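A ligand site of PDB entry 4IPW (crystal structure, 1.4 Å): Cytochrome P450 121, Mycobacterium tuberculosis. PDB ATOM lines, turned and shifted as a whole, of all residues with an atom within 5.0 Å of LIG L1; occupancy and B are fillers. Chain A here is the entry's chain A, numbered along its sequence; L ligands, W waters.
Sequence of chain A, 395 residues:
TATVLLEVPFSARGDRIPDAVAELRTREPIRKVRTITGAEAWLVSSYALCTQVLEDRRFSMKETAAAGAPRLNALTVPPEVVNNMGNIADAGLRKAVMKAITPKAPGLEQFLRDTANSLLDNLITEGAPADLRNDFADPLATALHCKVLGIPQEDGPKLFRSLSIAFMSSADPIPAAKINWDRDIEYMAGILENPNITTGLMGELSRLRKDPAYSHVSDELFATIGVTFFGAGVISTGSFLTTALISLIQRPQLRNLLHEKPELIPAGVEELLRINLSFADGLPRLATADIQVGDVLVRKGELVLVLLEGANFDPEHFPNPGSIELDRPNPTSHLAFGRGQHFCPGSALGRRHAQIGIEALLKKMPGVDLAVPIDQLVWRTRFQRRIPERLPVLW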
ATOM      1  N   MET A  61      37.775 -20.778  -5.385  1.00  0.00           N
ATOM      2  CA  MET A  61      37.003 -19.637  -4.909  1.00  0.00           C
ATOM      3  C   MET A  61      36.293 -20.043  -3.597  1.00  0.00           C
ATOM      4  O   MET A  61      36.338 -19.318  -2.606  1.00  0.00           O
ATOM      5  CB  MET A  61      35.951 -19.185  -5.954  1.00  0.00           C
ATOM      6  CG  MET A  61      34.869 -18.179  -5.415  1.00  0.00           C
ATOM      7  SD  MET A  61      35.525 -16.628  -4.584  1.00  0.00           S
ATOM      8  CE  MET A  61      35.860 -15.630  -6.068  1.00  0.00           C
ATOM      9  N   THR A  76      30.590 -10.105   2.515  1.00  0.00           N
ATOM     10  CA  THR A  76      29.341  -9.332   2.591  1.00  0.00           C
ATOM     11  C   THR A  76      28.135 -10.203   2.285  1.00  0.00           C
ATOM     12  O   THR A  76      26.987  -9.727   2.293  1.00  0.00           O
ATOM     13  CB  THR A  76      29.342  -8.136   1.658  1.00  0.00           C
ATOM     14  OG1 THR A  76      29.380  -8.623   0.327  1.00  0.00           O
ATOM     15  CG2 THR A  76      30.522  -7.220   1.910  1.00  0.00           C
ATOM     16  N   VAL A  77      28.382 -11.520   2.061  1.00  0.00           N
ATOM     17  CA  VAL A  77      27.324 -12.494   1.798  1.00  0.00           C
ATOM     18  C   VAL A  77      27.543 -13.662   2.768  1.00  0.00           C
ATOM     19  O   VAL A  77      28.651 -13.837   3.293  1.00  0.00           O
ATOM     20  CB  VAL A  77      27.371 -12.991   0.313  1.00  0.00           C
ATOM     21  CG1 VAL A  77      27.088 -11.840  -0.666  1.00  0.00           C
ATOM     22  CG2 VAL A  77      28.694 -13.687  -0.042  1.00  0.00           C
ATOM     23  N   VAL A  81      27.322 -18.690  -0.050  1.00  0.00           N
ATOM     24  CA  VAL A  81      27.107 -17.955  -1.305  1.00  0.00           C
ATOM     25  C   VAL A  81      28.444 -17.734  -2.034  1.00  0.00           C
ATOM     26  O   VAL A  81      28.465 -17.491  -3.233  1.00  0.00           O
ATOM     27  CB  VAL A  81      26.330 -16.650  -1.000  1.00  0.00           C
ATOM     28  CG1 VAL A  81      26.060 -15.807  -2.261  1.00  0.00           C
ATOM     29  CG2 VAL A  81      24.978 -17.007  -0.348  1.00  0.00           C
ATOM     30  N   VAL A  82      29.567 -17.922  -1.322  1.00  0.00           N
ATOM     31  CA  VAL A  82      30.849 -17.842  -2.014  1.00  0.00           C
ATOM     32  C   VAL A  82      30.957 -19.025  -2.996  1.00  0.00           C
ATOM     33  O   VAL A  82      31.697 -18.935  -3.955  1.00  0.00           O
ATOM     34  CB  VAL A  82      32.006 -17.808  -0.996  1.00  0.00           C
ATOM     35  CG1 VAL A  82      33.357 -17.803  -1.703  1.00  0.00           C
ATOM     36  CG2 VAL A  82      31.870 -16.584  -0.100  1.00  0.00           C
ATOM     37  N   ASN A  84      28.314 -19.866  -4.876  1.00  0.00           N
ATOM     38  CA  ASN A  84      27.041 -19.705  -5.576  1.00  0.00           C
ATOM     39  C   ASN A  84      26.877 -20.503  -6.848  1.00  0.00           C
ATOM     40  O   ASN A  84      25.919 -21.263  -6.986  1.00  0.00           O
ATOM     41  CB  ASN A  84      26.784 -18.212  -5.870  1.00  0.00           C
ATOM     42  CG  ASN A  84      25.339 -17.879  -6.205  1.00  0.00           C
ATOM     43  OD1 ASN A  84      24.405 -18.428  -5.603  1.00  0.00           O
ATOM     44  ND2 ASN A  84      25.129 -16.915  -7.083  1.00  0.00           N
ATOM     45  N   ALA A 166      26.757  -3.630  -0.533  1.00  0.00           N
ATOM     46  CA  ALA A 166      26.882  -5.073  -0.800  1.00  0.00           C
ATOM     47  C   ALA A 166      28.196  -5.381  -1.514  1.00  0.00           C
ATOM     48  O   ALA A 166      28.772  -6.460  -1.330  1.00  0.00           O
ATOM     49  CB  ALA A 166      25.698  -5.539  -1.651  1.00  0.00           C
ATOM     50  N   PHE A 167      28.670  -4.420  -2.362  1.00  0.00           N
ATOM     51  CA  PHE A 167      29.910  -4.600  -3.092  1.00  0.00           C
ATOM     52  C   PHE A 167      31.087  -3.834  -2.481  1.00  0.00           C
ATOM     53  O   PHE A 167      32.111  -3.630  -3.138  1.00  0.00           O
ATOM     54  CB  PHE A 167      29.714  -4.352  -4.604  1.00  0.00           C
ATOM     55  CG  PHE A 167      29.032  -5.545  -5.239  1.00  0.00           C
ATOM     56  CD1 PHE A 167      27.654  -5.620  -5.284  1.00  0.00           C
ATOM     57  CD2 PHE A 167      29.785  -6.627  -5.695  1.00  0.00           C
ATOM     58  CE1 PHE A 167      27.013  -6.773  -5.802  1.00  0.00           C
ATOM     59  CE2 PHE A 167      29.148  -7.777  -6.205  1.00  0.00           C
ATOM     60  CZ  PHE A 167      27.774  -7.826  -6.262  1.00  0.00           C
ATOM     61  N   TRP A 181      20.971  -7.664   2.858  1.00  0.00           N
ATOM     62  CA  TRP A 181      20.918  -9.035   2.291  1.00  0.00           C
ATOM     63  C   TRP A 181      19.646  -9.735   2.727  1.00  0.00           C
ATOM     64  O   TRP A 181      18.889 -10.276   1.904  1.00  0.00           O
ATOM     65  CB  TRP A 181      22.155  -9.835   2.753  1.00  0.00           C
ATOM     66  CG  TRP A 181      22.131 -11.260   2.289  1.00  0.00           C
ATOM     67  CD1 TRP A 181      21.699 -12.344   2.991  1.00  0.00           C
ATOM     68  CD2 TRP A 181      22.540 -11.739   1.003  1.00  0.00           C
ATOM     69  NE1 TRP A 181      21.770 -13.479   2.208  1.00  0.00           N
ATOM     70  CE2 TRP A 181      22.288 -13.138   0.980  1.00  0.00           C
ATOM     71  CE3 TRP A 181      23.095 -11.136  -0.139  1.00  0.00           C
ATOM     72  CZ2 TRP A 181      22.547 -13.943  -0.147  1.00  0.00           C
ATOM     73  CZ3 TRP A 181      23.362 -11.934  -1.249  1.00  0.00           C
ATOM     74  CH2 TRP A 181      23.082 -13.314  -1.243  1.00  0.00           C
ATOM     75  N   VAL A 227      18.817 -12.590  -5.846  1.00  0.00           N
ATOM     76  CA  VAL A 227      19.607 -11.484  -5.237  1.00  0.00           C
ATOM     77  C   VAL A 227      20.983 -11.364  -5.885  1.00  0.00           C
ATOM     78  O   VAL A 227      21.452 -10.254  -6.177  1.00  0.00           O
ATOM     79  CB  VAL A 227      19.714 -11.613  -3.673  1.00  0.00           C
ATOM     80  CG1 VAL A 227      20.605 -10.493  -3.072  1.00  0.00           C
ATOM     81  CG2 VAL A 227      18.347 -11.586  -3.044  1.00  0.00           C
ATOM     82  N   THR A 228      21.645 -12.517  -6.055  1.00  0.00           N
ATOM     83  CA  THR A 228      23.032 -12.503  -6.570  1.00  0.00           C
ATOM     84  C   THR A 228      23.120 -12.144  -8.038  1.00  0.00           C
ATOM     85  O   THR A 228      24.055 -11.419  -8.417  1.00  0.00           O
ATOM     86  CB  THR A 228      23.726 -13.826  -6.294  1.00  0.00           C
ATOM     87  OG1 THR A 228      23.000 -14.911  -6.931  1.00  0.00           O
ATOM     88  CG2 THR A 228      23.893 -14.103  -4.805  1.00  0.00           C
ATOM     89  N   GLY A 231      22.469  -8.429  -8.258  1.00  0.00           N
ATOM     90  CA  GLY A 231      23.557  -7.616  -7.694  1.00  0.00           C
ATOM     91  C   GLY A 231      24.804  -7.678  -8.548  1.00  0.00           C
ATOM     92  O   GLY A 231      25.355  -6.619  -8.942  1.00  0.00           O
ATOM     93  N   ALA A 232      25.322  -8.885  -8.828  1.00  0.00           N
ATOM     94  CA  ALA A 232      26.548  -8.963  -9.630  1.00  0.00           C
ATOM     95  C   ALA A 232      26.309  -8.386 -11.032  1.00  0.00           C
ATOM     96  O   ALA A 232      27.154  -7.658 -11.548  1.00  0.00           O
ATOM     97  CB  ALA A 232      27.017 -10.430  -9.744  1.00  0.00           C
ATOM     98  N   PHE A 279      37.378  -3.644 -12.105  1.00  0.00           N
ATOM     99  CA  PHE A 279      37.613  -4.509 -10.925  1.00  0.00           C
ATOM    100  C   PHE A 279      38.698  -3.894 -10.054  1.00  0.00           C
ATOM    101  O   PHE A 279      39.854  -3.725 -10.486  1.00  0.00           O
ATOM    102  CB  PHE A 279      37.956  -5.953 -11.332  1.00  0.00           C
ATOM    103  CG  PHE A 279      36.716  -6.788 -11.577  1.00  0.00           C
ATOM    104  CD1 PHE A 279      35.862  -6.489 -12.641  1.00  0.00           C
ATOM    105  CD2 PHE A 279      36.413  -7.870 -10.760  1.00  0.00           C
ATOM    106  CE1 PHE A 279      34.729  -7.279 -12.873  1.00  0.00           C
ATOM    107  CE2 PHE A 279      35.233  -8.622 -10.974  1.00  0.00           C
ATOM    108  CZ  PHE A 279      34.415  -8.315 -12.035  1.00  0.00           C
ATOM    109  N   GLN A 384      34.451  -2.981  -4.441  1.00  0.00           N
ATOM    110  CA  GLN A 384      34.877  -4.067  -5.330  1.00  0.00           C
ATOM    111  C   GLN A 384      34.972  -3.616  -6.769  1.00  0.00           C
ATOM    112  O   GLN A 384      35.507  -4.355  -7.605  1.00  0.00           O
ATOM    113  CB  GLN A 384      33.962  -5.280  -5.208  1.00  0.00           C
ATOM    114  CG  GLN A 384      34.106  -5.973  -3.843  1.00  0.00           C
ATOM    115  CD  GLN A 384      33.096  -7.064  -3.595  1.00  0.00           C
ATOM    116  OE1 GLN A 384      32.504  -7.177  -2.473  1.00  0.00           O
ATOM    117  NE2 GLN A 384      32.866  -7.876  -4.592  1.00  0.00           N
ATOM    118  N   ARG A 385      34.472  -2.397  -7.058  1.00  0.00           N
ATOM    119  CA  ARG A 385      34.611  -1.803  -8.375  1.00  0.00           C
ATOM    120  C   ARG A 385      35.246  -0.432  -8.240  1.00  0.00           C
ATOM    121  O   ARG A 385      35.148   0.198  -7.188  1.00  0.00           O
ATOM    122  CB  ARG A 385      33.245  -1.627  -9.073  1.00  0.00           C
ATOM    123  CG  ARG A 385      32.521  -2.958  -9.407  1.00  0.00           C
ATOM    124  CD  ARG A 385      33.318  -3.803 -10.444  1.00  0.00           C
ATOM    125  NE  ARG A 385      32.599  -5.036 -10.761  1.00  0.00           N
ATOM    126  CZ  ARG A 385      32.625  -6.121  -9.982  1.00  0.00           C
ATOM    127  NH1 ARG A 385      31.885  -7.197 -10.283  1.00  0.00           N
ATOM    128  NH2 ARG A 385      33.416  -6.156  -8.902  1.00  0.00           N
HETATM  129  O1  LIG L   1      27.570 -15.293  -7.465  1.00  0.00           O
HETATM  130  C1  LIG L   1      28.391 -15.090  -6.556  1.00  0.00           C
HETATM  131  C2  LIG L   1      28.104 -13.973  -5.580  1.00  0.00           C
HETATM  132  C3  LIG L   1      28.225 -12.578  -6.321  1.00  0.00           C
HETATM  133  C4  LIG L   1      27.612 -11.507  -5.384  1.00  0.00           C
HETATM  134  C5  LIG L   1      28.447 -10.801  -4.454  1.00  0.00           C
HETATM  135  C6  LIG L   1      27.868  -9.911  -3.599  1.00  0.00           C
HETATM  136  O2  LIG L   1      28.661  -9.188  -2.716  1.00  0.00           O
HETATM  137  C7  LIG L   1      26.501  -9.647  -3.612  1.00  0.00           C
HETATM  138  O3  LIG L   1      25.946  -8.758  -2.685  1.00  0.00           O
HETATM  139  C8  LIG L   1      25.658 -10.294  -4.586  1.00  0.00           C
HETATM  140  C9  LIG L   1      26.265 -11.222  -5.485  1.00  0.00           C
HETATM  141  N1  LIG L   1      28.992 -13.944  -4.408  1.00  0.00           N
HETATM  142  C10 LIG L   1      30.093 -14.666  -4.221  1.00  0.00           C
HETATM  143  O4  LIG L   1      30.811 -14.593  -3.198  1.00  0.00           O
HETATM  144  N2  LIG L   1      29.476 -15.831  -6.366  1.00  0.00           N
HETATM  145  C11 LIG L   1      30.489 -15.674  -5.306  1.00  0.00           C
HETATM  146  C12 LIG L   1      31.832 -15.266  -5.903  1.00  0.00           C
HETATM  147  C13 LIG L   1      31.780 -13.909  -6.594  1.00  0.00           C
HETATM  148  C14 LIG L   1      31.382 -13.721  -7.901  1.00  0.00           C
HETATM  149  C15 LIG L   1      31.301 -12.500  -8.580  1.00  0.00           C
HETATM  150  C16 LIG L   1      31.649 -11.335  -7.832  1.00  0.00           C
HETATM  151  O5  LIG L   1      31.600 -10.129  -8.438  1.00  0.00           O
HETATM  152  C17 LIG L   1      32.041 -11.507  -6.493  1.00  0.00           C
HETATM  153  C18 LIG L   1      32.098 -12.749  -5.865  1.00  0.00           C
HETATM  154  C1  LG2 L   2      31.736 -13.726 -12.468  1.00  0.00           C
HETATM  155  C2  LG2 L   2      33.023  -9.718 -14.894  1.00  0.00           C
HETATM  156  C3  LG2 L   2      28.354  -9.014 -16.078  1.00  0.00           C
HETATM  157  C4  LG2 L   2      27.028 -12.561 -13.044  1.00  0.00           C
HETATM  158  C5  LG2 L   2      32.512 -12.761 -13.119  1.00  0.00           C
HETATM  159  C6  LG2 L   2      33.941 -12.745 -13.158  1.00  0.00           C
HETATM  160  C7  LG2 L   2      34.297 -11.575 -13.776  1.00  0.00           C
HETATM  161  C8  LG2 L   2      33.100 -10.904 -14.192  1.00  0.00           C
HETATM  162  C9  LG2 L   2      35.718 -11.070 -14.013  1.00  0.00           C
HETATM  163  C10 LG2 L   2      34.868 -13.825 -12.562  1.00  0.00           C
HETATM  164  C11 LG2 L   2      35.059 -13.738 -11.057  1.00  0.00           C
HETATM  165  C12 LG2 L   2      36.063 -14.722 -10.586  1.00  0.00           C
HETATM  166  O1  LG2 L   2      36.536 -15.577 -11.333  1.00  0.00           O
HETATM  167  O2  LG2 L   2      36.366 -14.602  -9.301  1.00  0.00           O
HETATM  168  C13 LG2 L   2      31.815  -9.120 -15.369  1.00  0.00           C
HETATM  169  C14 LG2 L   2      31.819  -7.957 -16.230  1.00  0.00           C
HETATM  170  C15 LG2 L   2      30.492  -7.779 -16.592  1.00  0.00           C
HETATM  171  C16 LG2 L   2      29.751  -8.835 -15.885  1.00  0.00           C
HETATM  172  C17 LG2 L   2      33.033  -7.172 -16.626  1.00  0.00           C
HETATM  173  C18 LG2 L   2      29.856  -6.787 -17.480  1.00  0.00           C
HETATM  174  C19 LG2 L   2      30.461  -5.919 -18.246  1.00  0.00           C
HETATM  175  C20 LG2 L   2      27.603  -9.954 -15.414  1.00  0.00           C
HETATM  176  C21 LG2 L   2      26.165 -10.086 -15.547  1.00  0.00           C
HETATM  177  C22 LG2 L   2      25.788 -11.082 -14.671  1.00  0.00           C
HETATM  178  C23 LG2 L   2      26.999 -11.576 -14.028  1.00  0.00           C
HETATM  179  C24 LG2 L   2      25.277  -9.286 -16.472  1.00  0.00           C
HETATM  180  C25 LG2 L   2      24.424 -11.656 -14.398  1.00  0.00           C
HETATM  181  C26 LG2 L   2      23.282 -11.154 -14.817  1.00  0.00           C
HETATM  182  C27 LG2 L   2      28.202 -13.096 -12.566  1.00  0.00           C
HETATM  183  C28 LG2 L   2      28.252 -14.234 -11.635  1.00  0.00           C
HETATM  184  C29 LG2 L   2      29.550 -14.650 -11.586  1.00  0.00           C
HETATM  185  C30 LG2 L   2      30.328 -13.692 -12.413  1.00  0.00           C
HETATM  186  C31 LG2 L   2      27.054 -14.842 -10.941  1.00  0.00           C
HETATM  187  C32 LG2 L   2      30.179 -15.814 -10.778  1.00  0.00           C
HETATM  188  C33 LG2 L   2      30.435 -17.029 -11.687  1.00  0.00           C
HETATM  189  C34 LG2 L   2      31.121 -18.257 -11.104  1.00  0.00           C
HETATM  190  O3  LG2 L   2      31.222 -19.274 -11.749  1.00  0.00           O
HETATM  191  O4  LG2 L   2      31.591 -18.089  -9.896  1.00  0.00           O
HETATM  192  N1  LG2 L   2      31.971 -11.661 -13.801  1.00  0.00           N
HETATM  193  N2  LG2 L   2      30.575  -9.613 -15.164  1.00  0.00           N
HETATM  194  N3  LG2 L   2      28.082 -10.896 -14.543  1.00  0.00           N
HETATM  195  N4  LG2 L   2      29.501 -12.789 -12.971  1.00  0.00           N
HETATM  196 FE1  LG2 L   2      30.026 -11.343 -14.258  1.00  0.00          FE
HETATM  197  O   HOH W   1      31.625 -12.237  -2.184  1.00  0.00           O
HETATM  198  O   HOH W   2      33.556  -8.450  -7.227  1.00  0.00           O
HETATM  199  O   HOH W   3      31.290  -9.726  -3.181  1.00  0.00           O
HETATM  200  O   HOH W   4      32.244 -10.377 -10.902  1.00  0.00           O
HETATM  201  O   HOH W   5      25.832  -8.305   0.163  1.00  0.00           O
HETATM  202  O   HOH W   6      23.420  -8.130  -2.969  1.00  0.00           O
HETATM  203  O   HOH W   7      30.034 -18.350  -7.708  1.00  0.00           O
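An oxygen (O1) of LIG L1 is in hydrogen-bond range of the side-chain amide nitrogen (ND2) of Asn 84. O2 of LIG L1 lies within hydrogen-bond range of O of Ala 166. O2 of LIG L1 lies within hydrogen-bond range of OG1 of Thr 76 (3.2 Å). An oxygen (O5) of LIG L1 lies within hydrogen-bond range of the guanidinium group (NH1) of Arg 385, 3.5 Å away.
The side-chain amide nitrogen (ND2) of Asn 84 lies within hydrogen-bond range of the side-chain hydroxyl (OG1) of Thr 228 (2.9 Å). The backbone carbonyl oxygen (O) of Ala 166 sits at hydrogen-bond distance from the side-chain hydroxyl (OG1) of Thr 76, 2.8 Å away. The backbone carbonyl oxygen (O) of Phe 167 is in hydrogen-bond range of the backbone NH (N) of Gln 384 (2.8 Å).
Val 77 touches LIG L1 (CG1 to C6, 3.6 Å). Val 81 touches LIG L1. CA of Val 82 touches O4 of LIG L1, 3.5 Å away. Phe 167 touches LIG L1. Thr 228 touches LIG L1 (CA to C9, 3.6 Å). Hydrophobic or aromatic side chains that line LIG L1: Val 77, Val 82, Ala 166 and Phe 167. Within 4 Å of LIG L1: Thr 76, Val 77, Val 81, Val 82, Asn 84, Ala 166, Phe 167, Thr 228 and Arg 385. The nearest printed residue that does not touch LIG L1 is Met 61 (4.05 Å).
Water W4 bridges O5 of LIG L1 (2.6 Å) and NH1 of Arg 385 (3.3 Å). Water W3 bridges an oxygen (O2) of LIG L1 and the side-chain amide nitrogen of Gln 384. Water W2 lies within hydrogen-bond range of the side-chain amide nitrogen of Gln 384 (2.8 Å), the guanidinium group of Arg 385 (2.8 Å) and an oxygen (O5) of LIG L1 (2.8 Å). Water W5 bridges O of Thr 76 (2.8 Å) and O3 of LIG L1 (2.9 Å). Water W7 lies within hydrogen-bond range of an oxygen (O4) of LG2 L2 (2.7 Å) and a nitrogen (N2) of LIG L1 (2.9 Å).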
